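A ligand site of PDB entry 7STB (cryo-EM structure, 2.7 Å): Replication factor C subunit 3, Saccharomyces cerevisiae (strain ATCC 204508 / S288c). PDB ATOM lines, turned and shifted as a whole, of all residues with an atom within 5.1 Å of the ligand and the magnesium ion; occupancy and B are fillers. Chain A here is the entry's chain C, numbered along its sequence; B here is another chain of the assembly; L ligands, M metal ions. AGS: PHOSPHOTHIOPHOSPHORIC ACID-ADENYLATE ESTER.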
ATOM      1  N   TRP A  15      18.265 -19.351  16.757  1.00  0.00           N
ATOM      2  CA  TRP A  15      17.417 -18.389  16.063  1.00  0.00           C
ATOM      3  C   TRP A  15      17.892 -18.150  14.632  1.00  0.00           C
ATOM      4  O   TRP A  15      17.076 -17.848  13.763  1.00  0.00           O
ATOM      5  CB  TRP A  15      17.372 -17.076  16.831  1.00  0.00           C
ATOM      6  CG  TRP A  15      16.715 -17.170  18.178  1.00  0.00           C
ATOM      7  CD1 TRP A  15      16.357 -18.323  18.831  1.00  0.00           C
ATOM      8  CD2 TRP A  15      16.332 -16.094  19.023  1.00  0.00           C
ATOM      9  NE1 TRP A  15      15.774 -18.004  20.036  1.00  0.00           N
ATOM     10  CE2 TRP A  15      15.754 -16.645  20.181  1.00  0.00           C
ATOM     11  CE3 TRP A  15      16.428 -14.698  18.926  1.00  0.00           C
ATOM     12  CZ2 TRP A  15      15.260 -15.859  21.222  1.00  0.00           C
ATOM     13  CZ3 TRP A  15      15.938 -13.928  19.960  1.00  0.00           C
ATOM     14  CH2 TRP A  15      15.368 -14.512  21.095  1.00  0.00           C
ATOM     15  N   VAL A  16      19.193 -18.273  14.379  1.00  0.00           N
ATOM     16  CA  VAL A  16      19.703 -18.106  13.019  1.00  0.00           C
ATOM     17  C   VAL A  16      19.131 -19.155  12.082  1.00  0.00           C
ATOM     18  O   VAL A  16      19.116 -18.952  10.867  1.00  0.00           O
ATOM     19  CB  VAL A  16      21.249 -18.150  13.010  1.00  0.00           C
ATOM     20  CG1 VAL A  16      21.808 -16.887  13.631  1.00  0.00           C
ATOM     21  CG2 VAL A  16      21.759 -19.391  13.730  1.00  0.00           C
ATOM     22  N   GLU A  17      18.663 -20.285  12.624  1.00  0.00           N
ATOM     23  CA  GLU A  17      18.051 -21.335  11.825  1.00  0.00           C
ATOM     24  C   GLU A  17      16.556 -21.489  12.050  1.00  0.00           C
ATOM     25  O   GLU A  17      15.836 -21.853  11.122  1.00  0.00           O
ATOM     26  CB  GLU A  17      18.725 -22.678  12.102  1.00  0.00           C
ATOM     27  CG  GLU A  17      20.220 -22.669  11.850  1.00  0.00           C
ATOM     28  CD  GLU A  17      20.577 -23.160  10.461  1.00  0.00           C
ATOM     29  OE1 GLU A  17      21.678 -23.707  10.285  1.00  0.00           O
ATOM     30  OE2 GLU A  17      19.747 -22.982   9.550  1.00  0.00           O
ATOM     31  N   TYR A  19      14.517 -19.029  12.538  1.00  0.00           N
ATOM     32  CA  TYR A  19      13.915 -17.924  11.796  1.00  0.00           C
ATOM     33  C   TYR A  19      14.417 -17.852  10.361  1.00  0.00           C
ATOM     34  O   TYR A  19      14.462 -16.762   9.764  1.00  0.00           O
ATOM     35  CB  TYR A  19      14.188 -16.600  12.524  1.00  0.00           C
ATOM     36  CG  TYR A  19      13.500 -16.507  13.869  1.00  0.00           C
ATOM     37  CD1 TYR A  19      12.128 -16.324  13.967  1.00  0.00           C
ATOM     38  CD2 TYR A  19      14.235 -16.608  15.044  1.00  0.00           C
ATOM     39  CE1 TYR A  19      11.508 -16.243  15.193  1.00  0.00           C
ATOM     40  CE2 TYR A  19      13.617 -16.523  16.280  1.00  0.00           C
ATOM     41  CZ  TYR A  19      12.252 -16.344  16.345  1.00  0.00           C
ATOM     42  OH  TYR A  19      11.632 -16.263  17.572  1.00  0.00           O
ATOM     43  N   ARG A  20      14.811 -18.979   9.789  1.00  0.00           N
ATOM     44  CA  ARG A  20      15.199 -19.004   8.390  1.00  0.00           C
ATOM     45  C   ARG A  20      13.952 -18.817   7.523  1.00  0.00           C
ATOM     46  O   ARG A  20      12.967 -19.546   7.699  1.00  0.00           O
ATOM     47  CB  ARG A  20      15.888 -20.331   8.046  1.00  0.00           C
ATOM     48  CG  ARG A  20      16.222 -20.491   6.574  1.00  0.00           C
ATOM     49  CD  ARG A  20      17.184 -21.644   6.339  1.00  0.00           C
ATOM     50  NE  ARG A  20      18.499 -21.392   6.927  1.00  0.00           N
ATOM     51  CZ  ARG A  20      19.524 -20.839   6.284  1.00  0.00           C
ATOM     52  NH1 ARG A  20      19.426 -20.463   5.018  1.00  0.00           N
ATOM     53  NH2 ARG A  20      20.677 -20.674   6.925  1.00  0.00           N
ATOM     54  N   PRO A  21      13.947 -17.865   6.595  1.00  0.00           N
ATOM     55  CA  PRO A  21      12.750 -17.667   5.768  1.00  0.00           C
ATOM     56  C   PRO A  21      12.323 -18.948   5.059  1.00  0.00           C
ATOM     57  O   PRO A  21      13.142 -19.674   4.498  1.00  0.00           O
ATOM     58  CB  PRO A  21      13.204 -16.593   4.764  1.00  0.00           C
ATOM     59  CG  PRO A  21      14.257 -15.837   5.468  1.00  0.00           C
ATOM     60  CD  PRO A  21      14.959 -16.821   6.362  1.00  0.00           C
ATOM     61  N   GLU A  26       8.955 -13.718   3.163  1.00  0.00           N
ATOM     62  CA  GLU A  26       9.671 -13.392   4.384  1.00  0.00           C
ATOM     63  C   GLU A  26      11.055 -12.805   4.125  1.00  0.00           C
ATOM     64  O   GLU A  26      11.707 -12.367   5.075  1.00  0.00           O
ATOM     65  CB  GLU A  26       9.797 -14.630   5.273  1.00  0.00           C
ATOM     66  CG  GLU A  26       8.501 -15.382   5.492  1.00  0.00           C
ATOM     67  CD  GLU A  26       8.701 -16.677   6.265  1.00  0.00           C
ATOM     68  OE1 GLU A  26       9.652 -16.747   7.061  1.00  0.00           O
ATOM     69  OE2 GLU A  26       7.903 -17.613   6.061  1.00  0.00           O
ATOM     70  N   VAL A  27      11.506 -12.787   2.880  1.00  0.00           N
ATOM     71  CA  VAL A  27      12.804 -12.208   2.535  1.00  0.00           C
ATOM     72  C   VAL A  27      12.642 -10.698   2.446  1.00  0.00           C
ATOM     73  O   VAL A  27      11.799 -10.204   1.701  1.00  0.00           O
ATOM     74  CB  VAL A  27      13.340 -12.789   1.224  1.00  0.00           C
ATOM     75  CG1 VAL A  27      14.691 -12.181   0.879  1.00  0.00           C
ATOM     76  CG2 VAL A  27      13.447 -14.304   1.316  1.00  0.00           C
ATOM     77  N   TYR A  28      13.469  -9.967   3.196  1.00  0.00           N
ATOM     78  CA  TYR A  28      13.408  -8.517   3.256  1.00  0.00           C
ATOM     79  C   TYR A  28      14.725  -7.916   2.813  1.00  0.00           C
ATOM     80  O   TYR A  28      15.793  -8.512   2.994  1.00  0.00           O
ATOM     81  CB  TYR A  28      13.070  -8.041   4.677  1.00  0.00           C
ATOM     82  CG  TYR A  28      11.796  -8.618   5.242  1.00  0.00           C
ATOM     83  CD1 TYR A  28      10.587  -8.469   4.563  1.00  0.00           C
ATOM     84  CD2 TYR A  28      11.789  -9.312   6.443  1.00  0.00           C
ATOM     85  CE1 TYR A  28       9.410  -8.993   5.079  1.00  0.00           C
ATOM     86  CE2 TYR A  28      10.622  -9.840   6.958  1.00  0.00           C
ATOM     87  CZ  TYR A  28       9.439  -9.677   6.278  1.00  0.00           C
ATOM     88  OH  TYR A  28       8.281 -10.208   6.792  1.00  0.00           O
ATOM     89  N   GLY A  53      27.375 -11.498  -3.158  1.00  0.00           N
ATOM     90  CA  GLY A  53      27.176 -10.627  -2.016  1.00  0.00           C
ATOM     91  C   GLY A  53      27.933 -11.056  -0.780  1.00  0.00           C
ATOM     92  O   GLY A  53      28.487 -12.161  -0.695  1.00  0.00           O
ATOM     93  N   PRO A  54      27.954 -10.182   0.227  1.00  0.00           N
ATOM     94  CA  PRO A  54      28.675 -10.499   1.467  1.00  0.00           C
ATOM     95  C   PRO A  54      27.911 -11.499   2.309  1.00  0.00           C
ATOM     96  O   PRO A  54      26.780 -11.881   1.982  1.00  0.00           O
ATOM     97  CB  PRO A  54      28.769  -9.132   2.166  1.00  0.00           C
ATOM     98  CG  PRO A  54      27.622  -8.349   1.638  1.00  0.00           C
ATOM     99  CD  PRO A  54      27.388  -8.825   0.234  1.00  0.00           C
ATOM    100  N   PRO A  55      28.503 -11.965   3.411  1.00  0.00           N
ATOM    101  CA  PRO A  55      27.846 -12.986   4.226  1.00  0.00           C
ATOM    102  C   PRO A  55      26.532 -12.509   4.826  1.00  0.00           C
ATOM    103  O   PRO A  55      26.374 -11.337   5.182  1.00  0.00           O
ATOM    104  CB  PRO A  55      28.878 -13.283   5.326  1.00  0.00           C
ATOM    105  CG  PRO A  55      30.183 -12.810   4.778  1.00  0.00           C
ATOM    106  CD  PRO A  55      29.857 -11.637   3.911  1.00  0.00           C
ATOM    107  N   GLY A  56      25.589 -13.435   4.930  1.00  0.00           N
ATOM    108  CA  GLY A  56      24.341 -13.169   5.640  1.00  0.00           C
ATOM    109  C   GLY A  56      23.471 -12.106   5.014  1.00  0.00           C
ATOM    110  O   GLY A  56      22.933 -11.258   5.731  1.00  0.00           O
ATOM    111  N   THR A  57      23.301 -12.143   3.696  1.00  0.00           N
ATOM    112  CA  THR A  57      22.419 -11.216   3.000  1.00  0.00           C
ATOM    113  C   THR A  57      21.160 -11.878   2.460  1.00  0.00           C
ATOM    114  O   THR A  57      20.280 -11.163   1.963  1.00  0.00           O
ATOM    115  CB  THR A  57      23.167 -10.539   1.838  1.00  0.00           C
ATOM    116  OG1 THR A  57      23.592 -11.524   0.889  1.00  0.00           O
ATOM    117  CG2 THR A  57      24.369  -9.758   2.350  1.00  0.00           C
ATOM    118  N   GLY A  58      21.040 -13.190   2.556  1.00  0.00           N
ATOM    119  CA  GLY A  58      19.860 -13.901   2.123  1.00  0.00           C
ATOM    120  C   GLY A  58      19.959 -14.567   0.773  1.00  0.00           C
ATOM    121  O   GLY A  58      18.923 -14.728   0.116  1.00  0.00           O
ATOM    122  N   LYS A  59      21.157 -14.973   0.347  1.00  0.00           N
ATOM    123  CA  LYS A  59      21.293 -15.646  -0.934  1.00  0.00           C
ATOM    124  C   LYS A  59      20.827 -17.095  -0.857  1.00  0.00           C
ATOM    125  O   LYS A  59      19.991 -17.528  -1.651  1.00  0.00           O
ATOM    126  CB  LYS A  59      22.754 -15.578  -1.403  1.00  0.00           C
ATOM    127  CG  LYS A  59      23.338 -14.179  -1.402  1.00  0.00           C
ATOM    128  CD  LYS A  59      24.702 -14.145  -2.086  1.00  0.00           C
ATOM    129  CE  LYS A  59      25.794 -14.733  -1.193  1.00  0.00           C
ATOM    130  NZ  LYS A  59      26.059 -13.883  -0.005  1.00  0.00           N
ATOM    131  N   THR A  60      21.358 -17.854   0.108  1.00  0.00           N
ATOM    132  CA  THR A  60      20.917 -19.228   0.283  1.00  0.00           C
ATOM    133  C   THR A  60      19.436 -19.284   0.623  1.00  0.00           C
ATOM    134  O   THR A  60      18.693 -20.108   0.068  1.00  0.00           O
ATOM    135  CB  THR A  60      21.741 -19.913   1.375  1.00  0.00           C
ATOM    136  OG1 THR A  60      23.134 -19.679   1.134  1.00  0.00           O
ATOM    137  CG2 THR A  60      21.475 -21.413   1.392  1.00  0.00           C
ATOM    138  N   SER A  61      18.987 -18.420   1.531  1.00  0.00           N
ATOM    139  CA  SER A  61      17.568 -18.390   1.884  1.00  0.00           C
ATOM    140  C   SER A  61      16.709 -18.046   0.665  1.00  0.00           C
ATOM    141  O   SER A  61      15.673 -18.676   0.432  1.00  0.00           O
ATOM    142  CB  SER A  61      17.330 -17.373   2.997  1.00  0.00           C
ATOM    143  OG  SER A  61      17.976 -17.774   4.194  1.00  0.00           O
ATOM    144  N   THR A  62      17.136 -17.056  -0.122  1.00  0.00           N
ATOM    145  CA  THR A  62      16.359 -16.647  -1.283  1.00  0.00           C
ATOM    146  C   THR A  62      16.250 -17.776  -2.294  1.00  0.00           C
ATOM    147  O   THR A  62      15.175 -18.056  -2.828  1.00  0.00           O
ATOM    148  CB  THR A  62      16.970 -15.409  -1.923  1.00  0.00           C
ATOM    149  OG1 THR A  62      16.900 -14.308  -1.004  1.00  0.00           O
ATOM    150  CG2 THR A  62      16.240 -15.042  -3.210  1.00  0.00           C
ATOM    151  N   ASP A 117      26.283 -23.565  -4.017  1.00  0.00           N
ATOM    152  CA  ASP A 117      26.545 -22.673  -2.896  1.00  0.00           C
ATOM    153  C   ASP A 117      28.051 -22.568  -2.645  1.00  0.00           C
ATOM    154  O   ASP A 117      28.784 -23.558  -2.755  1.00  0.00           O
ATOM    155  CB  ASP A 117      25.837 -23.169  -1.641  1.00  0.00           C
ATOM    156  CG  ASP A 117      25.396 -22.030  -0.740  1.00  0.00           C
ATOM    157  OD1 ASP A 117      26.065 -20.976  -0.729  1.00  0.00           O
ATOM    158  OD2 ASP A 117      24.385 -22.191  -0.026  1.00  0.00           O
ATOM    159  N   GLU A 118      28.497 -21.370  -2.300  1.00  0.00           N
ATOM    160  CA  GLU A 118      29.909 -21.103  -2.050  1.00  0.00           C
ATOM    161  C   GLU A 118      30.771 -21.581  -3.219  1.00  0.00           C
ATOM    162  O   GLU A 118      31.796 -22.242  -3.039  1.00  0.00           O
ATOM    163  CB  GLU A 118      30.369 -21.739  -0.744  1.00  0.00           C
ATOM    164  CG  GLU A 118      29.672 -21.204   0.499  1.00  0.00           C
ATOM    165  CD  GLU A 118      28.536 -22.098   0.988  1.00  0.00           C
ATOM    166  OE1 GLU A 118      27.613 -21.577   1.629  1.00  0.00           O
ATOM    167  OE2 GLU A 118      28.591 -23.320   0.737  1.00  0.00           O
ATOM    168  N   LEU A 146      26.236 -19.057  -6.008  1.00  0.00           N
ATOM    169  CA  LEU A 146      26.292 -18.116  -4.890  1.00  0.00           C
ATOM    170  C   LEU A 146      27.755 -17.852  -4.554  1.00  0.00           C
ATOM    171  O   LEU A 146      28.550 -18.793  -4.436  1.00  0.00           O
ATOM    172  CB  LEU A 146      25.549 -18.672  -3.673  1.00  0.00           C
ATOM    173  CG  LEU A 146      24.022 -18.639  -3.761  1.00  0.00           C
ATOM    174  CD1 LEU A 146      23.512 -19.719  -4.701  1.00  0.00           C
ATOM    175  CD2 LEU A 146      23.430 -18.803  -2.373  1.00  0.00           C
ATOM    176  N   ASN A 148      30.711 -14.870  -2.571  1.00  0.00           N
ATOM    177  CA  ASN A 148      31.092 -13.663  -1.860  1.00  0.00           C
ATOM    178  C   ASN A 148      32.315 -12.980  -2.449  1.00  0.00           C
ATOM    179  O   ASN A 148      32.557 -11.806  -2.149  1.00  0.00           O
ATOM    180  CB  ASN A 148      31.373 -13.974  -0.376  1.00  0.00           C
ATOM    181  CG  ASN A 148      30.258 -14.764   0.279  1.00  0.00           C
ATOM    182  OD1 ASN A 148      30.067 -15.949  -0.008  1.00  0.00           O
ATOM    183  ND2 ASN A 148      29.520 -14.115   1.159  1.00  0.00           N
ATOM    184  N   LEU A 169      21.841  -5.472   3.888  1.00  0.00           N
ATOM    185  CA  LEU A 169      20.428  -5.320   4.187  1.00  0.00           C
ATOM    186  C   LEU A 169      20.150  -3.885   4.664  1.00  0.00           C
ATOM    187  O   LEU A 169      20.842  -3.409   5.571  1.00  0.00           O
ATOM    188  CB  LEU A 169      19.982  -6.320   5.240  1.00  0.00           C
ATOM    189  CG  LEU A 169      19.987  -7.786   4.789  1.00  0.00           C
ATOM    190  CD1 LEU A 169      19.760  -8.714   5.964  1.00  0.00           C
ATOM    191  CD2 LEU A 169      18.946  -8.015   3.704  1.00  0.00           C
ATOM    192  N   ARG A 177      12.337  -7.384  10.277  1.00  0.00           N
ATOM    193  CA  ARG A 177      12.615  -8.751  10.703  1.00  0.00           C
ATOM    194  C   ARG A 177      12.722  -8.838  12.225  1.00  0.00           C
ATOM    195  O   ARG A 177      12.290  -9.820  12.828  1.00  0.00           O
ATOM    196  CB  ARG A 177      13.898  -9.274  10.049  1.00  0.00           C
ATOM    197  CG  ARG A 177      14.053 -10.797  10.015  1.00  0.00           C
ATOM    198  CD  ARG A 177      12.799 -11.505   9.479  1.00  0.00           C
ATOM    199  NE  ARG A 177      13.002 -12.932   9.273  1.00  0.00           N
ATOM    200  CZ  ARG A 177      12.197 -13.894   9.703  1.00  0.00           C
ATOM    201  NH1 ARG A 177      11.086 -13.619  10.369  1.00  0.00           N
ATOM    202  NH2 ARG A 177      12.503 -15.163   9.466  1.00  0.00           N
ATOM    203  N   MET A 205      22.343 -10.134   8.929  1.00  0.00           N
ATOM    204  CA  MET A 205      21.203 -10.627   9.695  1.00  0.00           C
ATOM    205  C   MET A 205      21.611 -11.721  10.680  1.00  0.00           C
ATOM    206  O   MET A 205      20.987 -11.850  11.740  1.00  0.00           O
ATOM    207  CB  MET A 205      20.129 -11.150   8.747  1.00  0.00           C
ATOM    208  CG  MET A 205      18.821 -11.517   9.422  1.00  0.00           C
ATOM    209  SD  MET A 205      18.026 -10.115  10.238  1.00  0.00           S
ATOM    210  CE  MET A 205      17.382  -9.235   8.816  1.00  0.00           C
ATOM    211  N   ARG A 206      22.622 -12.515  10.347  1.00  0.00           N
ATOM    212  CA  ARG A 206      23.104 -13.530  11.278  1.00  0.00           C
ATOM    213  C   ARG A 206      23.554 -12.891  12.582  1.00  0.00           C
ATOM    214  O   ARG A 206      23.245 -13.381  13.673  1.00  0.00           O
ATOM    215  CB  ARG A 206      24.243 -14.330  10.661  1.00  0.00           C
ATOM    216  CG  ARG A 206      23.801 -15.477   9.772  1.00  0.00           C
ATOM    217  CD  ARG A 206      24.981 -16.053   9.018  1.00  0.00           C
ATOM    218  NE  ARG A 206      24.585 -17.120   8.113  1.00  0.00           N
ATOM    219  CZ  ARG A 206      25.256 -17.466   7.017  1.00  0.00           C
ATOM    220  NH1 ARG A 206      26.366 -16.845   6.667  1.00  0.00           N
ATOM    221  NH2 ARG A 206      24.795 -18.458   6.253  1.00  0.00           N
ATOM    222  N   LEU A 209      20.429 -11.838  14.612  1.00  0.00           N
ATOM    223  CA  LEU A 209      19.753 -12.938  15.296  1.00  0.00           C
ATOM    224  C   LEU A 209      20.584 -13.466  16.452  1.00  0.00           C
ATOM    225  O   LEU A 209      20.053 -13.735  17.539  1.00  0.00           O
ATOM    226  CB  LEU A 209      19.419 -14.047  14.305  1.00  0.00           C
ATOM    227  CG  LEU A 209      18.392 -13.683  13.235  1.00  0.00           C
ATOM    228  CD1 LEU A 209      18.345 -14.729  12.140  1.00  0.00           C
ATOM    229  CD2 LEU A 209      17.012 -13.499  13.861  1.00  0.00           C
ATOM    230  N   ARG B 154      31.386 -24.254   6.689  1.00  0.00           N
ATOM    231  CA  ARG B 154      30.313 -23.267   6.703  1.00  0.00           C
ATOM    232  C   ARG B 154      28.939 -23.924   6.681  1.00  0.00           C
ATOM    233  O   ARG B 154      28.142 -23.773   7.611  1.00  0.00           O
ATOM    234  CB  ARG B 154      30.465 -22.307   5.523  1.00  0.00           C
ATOM    235  CG  ARG B 154      31.489 -21.215   5.755  1.00  0.00           C
ATOM    236  CD  ARG B 154      31.832 -20.474   4.478  1.00  0.00           C
ATOM    237  NE  ARG B 154      30.720 -19.643   4.013  1.00  0.00           N
ATOM    238  CZ  ARG B 154      30.674 -19.019   2.848  1.00  0.00           C
ATOM    239  NH1 ARG B 154      31.679 -19.107   1.981  1.00  0.00           N
ATOM    240  NH2 ARG B 154      29.602 -18.298   2.530  1.00  0.00           N
ATOM    241  N   ARG B 155      28.644 -24.681   5.620  1.00  0.00           N
ATOM    242  CA  ARG B 155      27.311 -25.244   5.472  1.00  0.00           C
ATOM    243  C   ARG B 155      27.082 -26.441   6.392  1.00  0.00           C
ATOM    244  O   ARG B 155      25.946 -26.715   6.784  1.00  0.00           O
ATOM    245  CB  ARG B 155      27.051 -25.654   4.019  1.00  0.00           C
ATOM    246  CG  ARG B 155      26.742 -24.476   3.093  1.00  0.00           C
ATOM    247  CD  ARG B 155      25.412 -23.809   3.429  1.00  0.00           C
ATOM    248  NE  ARG B 155      24.270 -24.652   3.086  1.00  0.00           N
ATOM    249  CZ  ARG B 155      23.022 -24.414   3.472  1.00  0.00           C
ATOM    250  NH1 ARG B 155      22.715 -23.365   4.223  1.00  0.00           N
ATOM    251  NH2 ARG B 155      22.049 -25.252   3.101  1.00  0.00           N
ATOM    252  N   GLU B 158      25.520 -25.426   9.483  1.00  0.00           N
ATOM    253  CA  GLU B 158      24.123 -25.028   9.342  1.00  0.00           C
ATOM    254  C   GLU B 158      23.193 -26.192   9.027  1.00  0.00           C
ATOM    255  O   GLU B 158      22.090 -26.260   9.569  1.00  0.00           O
ATOM    256  CB  GLU B 158      23.996 -23.977   8.236  1.00  0.00           C
ATOM    257  CG  GLU B 158      24.295 -22.557   8.689  1.00  0.00           C
ATOM    258  CD  GLU B 158      24.262 -21.560   7.548  1.00  0.00           C
ATOM    259  OE1 GLU B 158      24.214 -21.998   6.381  1.00  0.00           O
ATOM    260  OE2 GLU B 158      24.293 -20.342   7.826  1.00  0.00           O
ATOM    261  N   PRO B 179      32.592 -15.505   6.988  1.00  0.00           N
ATOM    262  CA  PRO B 179      31.379 -16.336   7.044  1.00  0.00           C
ATOM    263  C   PRO B 179      31.237 -17.117   8.345  1.00  0.00           C
ATOM    264  O   PRO B 179      30.138 -17.206   8.893  1.00  0.00           O
ATOM    265  CB  PRO B 179      31.531 -17.264   5.834  1.00  0.00           C
ATOM    266  CG  PRO B 179      32.401 -16.515   4.891  1.00  0.00           C
ATOM    267  CD  PRO B 179      33.349 -15.737   5.739  1.00  0.00           C
ATOM    268  N   ARG B 183      28.407 -16.980  11.217  1.00  0.00           N
ATOM    269  CA  ARG B 183      27.618 -18.155  11.573  1.00  0.00           C
ATOM    270  C   ARG B 183      27.660 -18.482  13.060  1.00  0.00           C
ATOM    271  O   ARG B 183      26.839 -19.283  13.516  1.00  0.00           O
ATOM    272  CB  ARG B 183      28.098 -19.365  10.773  1.00  0.00           C
ATOM    273  CG  ARG B 183      27.481 -19.510   9.406  1.00  0.00           C
ATOM    274  CD  ARG B 183      28.198 -20.590   8.609  1.00  0.00           C
ATOM    275  NE  ARG B 183      27.584 -20.804   7.296  1.00  0.00           N
ATOM    276  CZ  ARG B 183      27.782 -20.030   6.243  1.00  0.00           C
ATOM    277  NH1 ARG B 183      28.540 -18.950   6.301  1.00  0.00           N
ATOM    278  NH2 ARG B 183      27.200 -20.358   5.091  1.00  0.00           N
HETATM  279  PG  AGS L   1      26.592 -16.577   3.151  1.00  0.00           P
HETATM  280  S1G AGS L   1      28.087 -16.653   4.400  1.00  0.00           S
HETATM  281  O2G AGS L   1      26.137 -18.019   2.803  1.00  0.00           O
HETATM  282  O3G AGS L   1      27.063 -15.860   1.853  1.00  0.00           O
HETATM  283  PB  AGS L   1      23.958 -15.869   3.166  1.00  0.00           P
HETATM  284  O1B AGS L   1      23.679 -14.666   2.354  1.00  0.00           O
HETATM  285  O2B AGS L   1      23.908 -17.162   2.347  1.00  0.00           O
HETATM  286  O3B AGS L   1      25.409 -15.788   3.792  1.00  0.00           O
HETATM  287  PA  AGS L   1      21.882 -17.258   4.314  1.00  0.00           P
HETATM  288  O1A AGS L   1      20.823 -17.064   3.297  1.00  0.00           O
HETATM  289  O2A AGS L   1      22.723 -18.523   4.099  1.00  0.00           O
HETATM  290  O3A AGS L   1      22.885 -16.035   4.325  1.00  0.00           O
HETATM  291  O5' AGS L   1      21.188 -17.266   5.737  1.00  0.00           O
HETATM  292  C5' AGS L   1      21.520 -16.287   6.739  1.00  0.00           C
HETATM  293  C4' AGS L   1      20.453 -16.283   7.798  1.00  0.00           C
HETATM  294  O4' AGS L   1      20.175 -14.921   8.202  1.00  0.00           O
HETATM  295  C3' AGS L   1      19.113 -16.870   7.358  1.00  0.00           C
HETATM  296  O3' AGS L   1      19.017 -18.248   7.697  1.00  0.00           O
HETATM  297  C2' AGS L   1      18.098 -16.035   8.130  1.00  0.00           C
HETATM  298  O2' AGS L   1      17.904 -16.510   9.460  1.00  0.00           O
HETATM  299  C1' AGS L   1      18.791 -14.665   8.138  1.00  0.00           C
HETATM  300  N9  AGS L   1      18.525 -13.865   6.941  1.00  0.00           N
HETATM  301  C8  AGS L   1      19.410 -13.554   5.946  1.00  0.00           C
HETATM  302  N7  AGS L   1      18.904 -12.819   4.995  1.00  0.00           N
HETATM  303  C5  AGS L   1      17.583 -12.637   5.383  1.00  0.00           C
HETATM  304  C6  AGS L   1      16.506 -11.943   4.795  1.00  0.00           C
HETATM  305  N6  AGS L   1      16.593 -11.277   3.641  1.00  0.00           N
HETATM  306  N1  AGS L   1      15.327 -11.957   5.443  1.00  0.00           N
HETATM  307  C2  AGS L   1      15.231 -12.620   6.598  1.00  0.00           C
HETATM  308  N3  AGS L   1      16.175 -13.316   7.248  1.00  0.00           N
HETATM  309  C4  AGS L   1      17.330 -13.278   6.586  1.00  0.00           C
HETATM  310 MG    MG M   1      24.793 -19.340   2.286  1.00  0.00          MG
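Residues that only touch the ligand: Leu 209 (3.2 Å), Met 205 (3.4 Å), Val 27 (3.5 Å), Arg 177 (3.5 Å), Pro 21 (3.5 Å), Pro 55 (3.6 Å), Glu 26 (3.7 Å), Pro 179 of chain B (3.8 Å) and Pro 54 (3.99 Å). Hydrophobic or aromatic side chains within 4 Å of the ligand: Pro 21, Val 27, Pro 55, Met 205, Leu 209 and Pro 179 of chain B. Within 4 Å of the ligand: Val 16, Tyr 19, Arg 20, Pro 21, Glu 26, Val 27, Tyr 28, Pro 54, Pro 55, Gly 56, Thr 57, Gly 58, Lys 59, Thr 60, Ser 61, Asn 148, Arg 177, Met 205, Arg 206, Leu 209, Arg 154 of chain B, Pro 179 of chain B and Arg 183 of chain B. The nearest printed residue that does not touch the ligand is Leu 169 (4.02 Å).
OD2 of Asp 117 sits close to OG1 of Thr 60 (3.0 Å). The guanidinium group (NH2) of Arg 206 is in salt-bridge range of the side-chain carboxylate (OE2) of Glu 158 of chain B. NZ of Lys 59 sits at hydrogen-bond distance from O of Pro 54 (2.9 Å). NE of Arg 183 of chain B sits at hydrogen-bond distance from O of Arg 154 of chain B. NH2 of Arg 154 of chain B lies within hydrogen-bond range of OD1 of Asn 148 (3.5 Å). NE of Arg 20 lies within salt-bridge range of OE2 of Glu 17 (3.3 Å). OE1 of Glu 118 lies within salt-bridge range of NH2 of Arg 183 of chain B. The backbone NH (N) of Glu 118 lies within hydrogen-bond range of the backbone carbonyl oxygen (O) of Leu 146, 3.3 Å away.
Asp 117 touches the magnesium ion (OD1 to MG, 3.7 Å). Glu 118 touches the magnesium ion. Arg 183 of chain B touches the magnesium ion (NH2 to MG, 3.8 Å). Within 4 Å of the magnesium ion: Thr 60, Asp 117, Glu 118 and Arg 183 of chain B. The nearest printed residue that does not touch the magnesium ion is Arg 206 (4.1 Å).
The backbone NH (N) of Thr 60 is in hydrogen-bond range of an oxygen (O1A) of the ligand (3.3 Å). The backbone NH (N) of Gly 56 sits at hydrogen-bond distance from an oxygen (O3B) of the ligand, 2.6 Å away. The guanidinium group of Arg 206 lies within salt-bridge range of an oxygen (O2A) of the ligand, 3.0 Å away. O1B of the ligand is in hydrogen-bond range of N of Thr 57, at 2.9 Å. O1B of the ligand is in hydrogen-bond range of OG1 of Thr 57 (3.5 Å). O1A of the ligand is in hydrogen-bond range of N of Ser 61 (2.9 Å). The side-chain hydroxyl of Ser 61 sits at hydrogen-bond distance from an oxygen (O1A) of the ligand. N of Lys 59 sits at hydrogen-bond distance from O1B of the ligand (3.2 Å). The side-chain amino group (NZ) of Lys 59 lies within salt-bridge range of an oxygen (O1B) of the ligand, at 3.4 Å. The guanidinium group (NH2) of Arg 154 of chain B lies close to a sulfur (S1G) of the ligand (2.9 Å). N6 of the ligand is in hydrogen-bond range of O of Tyr 28. The guanidinium group (NH1) of Arg 20 is in salt-bridge range of an oxygen (O2A) of the ligand (3.9 Å). S1G of the ligand lies close to NH1 of Arg 183 of chain B. An oxygen (O1B) of the ligand sits at hydrogen-bond distance from the backbone NH of Gly 58. O of Val 16 sits at hydrogen-bond distance from O2' of the ligand. The side-chain amide nitrogen of Asn 148 lies within hydrogen-bond range of an oxygen (O3G) of the ligand (3.1 Å). The backbone carbonyl oxygen (O) of Tyr 19 sits at hydrogen-bond distance from an oxygen (O2') of the ligand (3.5 Å).
The magnesium ion is bound by O2G of the ligand, OG1 of Thr 60 and O2B of the ligand.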
